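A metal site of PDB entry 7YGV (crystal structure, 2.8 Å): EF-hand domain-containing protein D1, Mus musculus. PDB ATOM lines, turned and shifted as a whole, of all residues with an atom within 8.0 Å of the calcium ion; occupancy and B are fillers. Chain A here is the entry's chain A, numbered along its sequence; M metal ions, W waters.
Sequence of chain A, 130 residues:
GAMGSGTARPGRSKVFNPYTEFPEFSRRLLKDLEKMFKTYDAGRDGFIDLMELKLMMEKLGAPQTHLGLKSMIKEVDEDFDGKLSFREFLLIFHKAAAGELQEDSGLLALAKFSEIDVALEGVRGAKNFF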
ATOM      1  N   PHE A  47     -16.864 -17.207  12.976  1.00  0.00           N
ATOM      2  CA  PHE A  47     -17.154 -16.029  13.765  1.00  0.00           C
ATOM      3  C   PHE A  47     -15.891 -15.170  13.798  1.00  0.00           C
ATOM      4  O   PHE A  47     -14.792 -15.681  13.602  1.00  0.00           O
ATOM      5  CB  PHE A  47     -17.558 -16.348  15.230  1.00  0.00           C
ATOM      6  CG  PHE A  47     -18.698 -17.303  15.368  1.00  0.00           C
ATOM      7  CD1 PHE A  47     -20.012 -16.838  15.311  1.00  0.00           C
ATOM      8  CD2 PHE A  47     -18.485 -18.648  15.625  1.00  0.00           C
ATOM      9  CE1 PHE A  47     -21.098 -17.715  15.439  1.00  0.00           C
ATOM     10  CE2 PHE A  47     -19.555 -19.521  15.771  1.00  0.00           C
ATOM     11  CZ  PHE A  47     -20.859 -19.057  15.684  1.00  0.00           C
ATOM     12  N   ILE A  48     -16.087 -13.882  14.066  1.00  0.00           N
ATOM     13  CA  ILE A  48     -15.005 -12.946  14.370  1.00  0.00           C
ATOM     14  C   ILE A  48     -15.173 -12.570  15.842  1.00  0.00           C
ATOM     15  O   ILE A  48     -16.175 -11.950  16.222  1.00  0.00           O
ATOM     16  CB  ILE A  48     -15.067 -11.717  13.448  1.00  0.00           C
ATOM     17  CG1 ILE A  48     -14.769 -12.118  11.993  1.00  0.00           C
ATOM     18  CG2 ILE A  48     -14.061 -10.631  13.897  1.00  0.00           C
ATOM     19  CD1 ILE A  48     -14.936 -10.967  10.984  1.00  0.00           C
ATOM     20  N   ILE A  73     -19.034  -4.843  19.082  1.00  0.00           N
ATOM     21  CA  ILE A  73     -19.742  -6.114  18.952  1.00  0.00           C
ATOM     22  C   ILE A  73     -21.132  -6.010  19.540  1.00  0.00           C
ATOM     23  O   ILE A  73     -22.115  -6.417  18.913  1.00  0.00           O
ATOM     24  CB  ILE A  73     -18.957  -7.259  19.613  1.00  0.00           C
ATOM     25  CG1 ILE A  73     -17.645  -7.513  18.867  1.00  0.00           C
ATOM     26  CG2 ILE A  73     -19.797  -8.526  19.591  1.00  0.00           C
ATOM     27  CD1 ILE A  73     -16.782  -8.616  19.470  1.00  0.00           C
ATOM     28  N   VAL A  76     -24.311  -4.997  17.490  1.00  0.00           N
ATOM     29  CA  VAL A  76     -24.849  -5.843  16.424  1.00  0.00           C
ATOM     30  C   VAL A  76     -24.888  -7.312  16.825  1.00  0.00           C
ATOM     31  O   VAL A  76     -25.085  -8.181  15.968  1.00  0.00           O
ATOM     32  CB  VAL A  76     -24.061  -5.641  15.108  1.00  0.00           C
ATOM     33  CG1 VAL A  76     -24.271  -4.219  14.554  1.00  0.00           C
ATOM     34  CG2 VAL A  76     -22.558  -5.942  15.313  1.00  0.00           C
ATOM     35  N   ASP A  77     -24.700  -7.609  18.116  1.00  0.00           N
ATOM     36  CA  ASP A  77     -24.621  -8.990  18.602  1.00  0.00           C
ATOM     37  C   ASP A  77     -26.042  -9.491  18.886  1.00  0.00           C
ATOM     38  O   ASP A  77     -26.504  -9.559  20.033  1.00  0.00           O
ATOM     39  CB  ASP A  77     -23.721  -9.076  19.827  1.00  0.00           C
ATOM     40  CG  ASP A  77     -23.406 -10.519  20.224  1.00  0.00           C
ATOM     41  OD1 ASP A  77     -23.473 -11.402  19.322  1.00  0.00           O
ATOM     42  OD2 ASP A  77     -23.128 -10.753  21.425  1.00  0.00           O
ATOM     43  N   GLU A  78     -26.749  -9.860  17.804  1.00  0.00           N
ATOM     44  CA  GLU A  78     -28.158 -10.227  17.937  1.00  0.00           C
ATOM     45  C   GLU A  78     -28.391 -11.556  18.637  1.00  0.00           C
ATOM     46  O   GLU A  78     -29.522 -11.801  19.082  1.00  0.00           O
ATOM     47  CB  GLU A  78     -28.816 -10.266  16.559  1.00  0.00           C
ATOM     48  CG  GLU A  78     -28.893  -8.924  15.870  1.00  0.00           C
ATOM     49  CD  GLU A  78     -29.434  -9.018  14.473  1.00  0.00           C
ATOM     50  OE1 GLU A  78     -29.137 -10.028  13.776  1.00  0.00           O
ATOM     51  OE2 GLU A  78     -30.173  -8.098  14.078  1.00  0.00           O
ATOM     52  N   ASP A  79     -27.398 -12.429  18.739  1.00  0.00           N
ATOM     53  CA  ASP A  79     -27.569 -13.682  19.465  1.00  0.00           C
ATOM     54  C   ASP A  79     -26.808 -13.674  20.782  1.00  0.00           C
ATOM     55  O   ASP A  79     -26.722 -14.721  21.438  1.00  0.00           O
ATOM     56  CB  ASP A  79     -27.166 -14.873  18.591  1.00  0.00           C
ATOM     57  CG  ASP A  79     -25.742 -14.791  18.111  1.00  0.00           C
ATOM     58  OD1 ASP A  79     -24.950 -14.043  18.714  1.00  0.00           O
ATOM     59  OD2 ASP A  79     -25.412 -15.456  17.106  1.00  0.00           O
ATOM     60  N   PHE A  80     -26.260 -12.537  21.188  1.00  0.00           N
ATOM     61  CA  PHE A  80     -25.751 -12.300  22.533  1.00  0.00           C
ATOM     62  C   PHE A  80     -24.534 -13.138  22.888  1.00  0.00           C
ATOM     63  O   PHE A  80     -24.297 -13.390  24.078  1.00  0.00           O
ATOM     64  CB  PHE A  80     -26.862 -12.521  23.576  1.00  0.00           C
ATOM     65  CG  PHE A  80     -28.067 -11.641  23.384  1.00  0.00           C
ATOM     66  CD1 PHE A  80     -28.092 -10.347  23.864  1.00  0.00           C
ATOM     67  CD2 PHE A  80     -29.172 -12.111  22.690  1.00  0.00           C
ATOM     68  CE1 PHE A  80     -29.189  -9.541  23.677  1.00  0.00           C
ATOM     69  CE2 PHE A  80     -30.276 -11.293  22.494  1.00  0.00           C
ATOM     70  CZ  PHE A  80     -30.279 -10.007  23.001  1.00  0.00           C
ATOM     71  N   ASP A  81     -23.738 -13.587  21.917  1.00  0.00           N
ATOM     72  CA  ASP A  81     -22.664 -14.528  22.228  1.00  0.00           C
ATOM     73  C   ASP A  81     -21.271 -13.896  22.312  1.00  0.00           C
ATOM     74  O   ASP A  81     -20.284 -14.630  22.470  1.00  0.00           O
ATOM     75  CB  ASP A  81     -22.641 -15.704  21.228  1.00  0.00           C
ATOM     76  CG  ASP A  81     -22.156 -15.302  19.832  1.00  0.00           C
ATOM     77  OD1 ASP A  81     -21.989 -14.106  19.534  1.00  0.00           O
ATOM     78  OD2 ASP A  81     -21.921 -16.215  19.033  1.00  0.00           O
ATOM     79  N   GLY A  82     -21.156 -12.574  22.204  1.00  0.00           N
ATOM     80  CA  GLY A  82     -19.875 -11.909  22.314  1.00  0.00           C
ATOM     81  C   GLY A  82     -19.033 -11.841  21.052  1.00  0.00           C
ATOM     82  O   GLY A  82     -18.015 -11.140  21.041  1.00  0.00           O
ATOM     83  N   LYS A  83     -19.429 -12.538  19.988  1.00  0.00           N
ATOM     84  CA  LYS A  83     -18.633 -12.567  18.766  1.00  0.00           C
ATOM     85  C   LYS A  83     -19.544 -12.280  17.569  1.00  0.00           C
ATOM     86  O   LYS A  83     -20.766 -12.169  17.730  1.00  0.00           O
ATOM     87  CB  LYS A  83     -17.895 -13.896  18.609  1.00  0.00           C
ATOM     88  CG  LYS A  83     -18.773 -15.109  18.837  1.00  0.00           C
ATOM     89  CD  LYS A  83     -17.944 -16.361  19.154  1.00  0.00           C
ATOM     90  CE  LYS A  83     -18.865 -17.577  19.197  1.00  0.00           C
ATOM     91  NZ  LYS A  83     -18.186 -18.801  19.680  1.00  0.00           N
ATOM     92  N   LEU A  84     -18.954 -12.182  16.368  1.00  0.00           N
ATOM     93  CA  LEU A  84     -19.696 -11.729  15.190  1.00  0.00           C
ATOM     94  C   LEU A  84     -19.902 -12.875  14.215  1.00  0.00           C
ATOM     95  O   LEU A  84     -18.945 -13.337  13.580  1.00  0.00           O
ATOM     96  CB  LEU A  84     -18.984 -10.567  14.469  1.00  0.00           C
ATOM     97  CG  LEU A  84     -18.642  -9.233  15.132  1.00  0.00           C
ATOM     98  CD1 LEU A  84     -17.772  -8.387  14.197  1.00  0.00           C
ATOM     99  CD2 LEU A  84     -19.880  -8.464  15.563  1.00  0.00           C
ATOM    100  N   SER A  85     -21.154 -13.274  14.037  1.00  0.00           N
ATOM    101  CA  SER A  85     -21.498 -14.144  12.924  1.00  0.00           C
ATOM    102  C   SER A  85     -21.419 -13.355  11.618  1.00  0.00           C
ATOM    103  O   SER A  85     -21.393 -12.115  11.594  1.00  0.00           O
ATOM    104  CB  SER A  85     -22.897 -14.742  13.118  1.00  0.00           C
ATOM    105  OG  SER A  85     -23.900 -13.734  13.056  1.00  0.00           O
ATOM    106  N   PHE A  86     -21.386 -14.082  10.503  1.00  0.00           N
ATOM    107  CA  PHE A  86     -21.399 -13.424   9.207  1.00  0.00           C
ATOM    108  C   PHE A  86     -22.590 -12.483   9.086  1.00  0.00           C
ATOM    109  O   PHE A  86     -22.433 -11.317   8.685  1.00  0.00           O
ATOM    110  CB  PHE A  86     -21.415 -14.455   8.084  1.00  0.00           C
ATOM    111  CG  PHE A  86     -21.305 -13.858   6.725  1.00  0.00           C
ATOM    112  CD1 PHE A  86     -20.301 -12.942   6.445  1.00  0.00           C
ATOM    113  CD2 PHE A  86     -22.208 -14.193   5.726  1.00  0.00           C
ATOM    114  CE1 PHE A  86     -20.188 -12.379   5.188  1.00  0.00           C
ATOM    115  CE2 PHE A  86     -22.103 -13.639   4.463  1.00  0.00           C
ATOM    116  CZ  PHE A  86     -21.084 -12.728   4.198  1.00  0.00           C
ATOM    117  N   ARG A  87     -23.798 -12.943   9.443  1.00  0.00           N
ATOM    118  CA  ARG A  87     -24.978 -12.098   9.260  1.00  0.00           C
ATOM    119  C   ARG A  87     -24.861 -10.815  10.069  1.00  0.00           C
ATOM    120  O   ARG A  87     -25.188  -9.728   9.571  1.00  0.00           O
ATOM    121  CB  ARG A  87     -26.276 -12.850   9.608  1.00  0.00           C
ATOM    122  CG  ARG A  87     -26.471 -13.199  11.074  1.00  0.00           C
ATOM    123  CD  ARG A  87     -27.643 -14.145  11.215  1.00  0.00           C
ATOM    124  NE  ARG A  87     -28.897 -13.503  10.847  1.00  0.00           N
ATOM    125  CZ  ARG A  87     -30.047 -14.135  10.675  1.00  0.00           C
ATOM    126  NH1 ARG A  87     -30.141 -15.446  10.817  1.00  0.00           N
ATOM    127  NH2 ARG A  87     -31.125 -13.437  10.336  1.00  0.00           N
ATOM    128  N   GLU A  88     -24.348 -10.910  11.304  1.00  0.00           N
ATOM    129  CA  GLU A  88     -24.129  -9.715  12.098  1.00  0.00           C
ATOM    130  C   GLU A  88     -23.016  -8.866  11.512  1.00  0.00           C
ATOM    131  O   GLU A  88     -23.106  -7.635  11.543  1.00  0.00           O
ATOM    132  CB  GLU A  88     -23.811 -10.093  13.546  1.00  0.00           C
ATOM    133  CG  GLU A  88     -24.902 -10.864  14.278  1.00  0.00           C
ATOM    134  CD  GLU A  88     -24.354 -11.541  15.522  1.00  0.00           C
ATOM    135  OE1 GLU A  88     -23.114 -11.748  15.559  1.00  0.00           O
ATOM    136  OE2 GLU A  88     -25.145 -11.863  16.438  1.00  0.00           O
ATOM    137  N   PHE A  89     -21.975  -9.490  10.955  1.00  0.00           N
ATOM    138  CA  PHE A  89     -20.976  -8.726  10.209  1.00  0.00           C
ATOM    139  C   PHE A  89     -21.651  -7.906   9.100  1.00  0.00           C
ATOM    140  O   PHE A  89     -21.486  -6.682   9.034  1.00  0.00           O
ATOM    141  CB  PHE A  89     -19.904  -9.648   9.631  1.00  0.00           C
ATOM    142  CG  PHE A  89     -18.742  -8.936   8.984  1.00  0.00           C
ATOM    143  CD1 PHE A  89     -17.846  -8.196   9.746  1.00  0.00           C
ATOM    144  CD2 PHE A  89     -18.518  -9.039   7.612  1.00  0.00           C
ATOM    145  CE1 PHE A  89     -16.767  -7.540   9.139  1.00  0.00           C
ATOM    146  CE2 PHE A  89     -17.451  -8.385   7.011  1.00  0.00           C
ATOM    147  CZ  PHE A  89     -16.578  -7.637   7.778  1.00  0.00           C
HETATM  148 CA    CA M   1     -23.114 -13.043  17.700  1.00  0.00          CA
HETATM  149  O   HOH W   1     -22.892 -15.089  16.920  1.00  0.00           O
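The backbone NH of Glu 78 lies close to the side-chain carboxylate of Glu 88.
The backbone NH of Glu 88 lies close to the side-chain hydroxyl of Ser 85.
The side-chain carboxylate (OD2) of Asp 77 lies within hydrogen-bond range of the backbone NH (N) of Gly 82 (2.8 Å).
Five residues have an atom within 4 Å of the calcium ion: Asp 77, Asp 79, Asp 81, Lys 83 and Glu 88.
The calcium ion is bound by water W1, OD1 of Asp 79, OD1 of Asp 77, OD1 of Asp 81, OE1 of Glu 88, O of Lys 83 and OE2 of Glu 88.
The calcium ion has seven donor atoms within binding distance.
Water W1 lies within hydrogen-bond range of OD2 of Asp 79 (2.6 Å) and OD2 of Asp 81 (2.6 Å).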
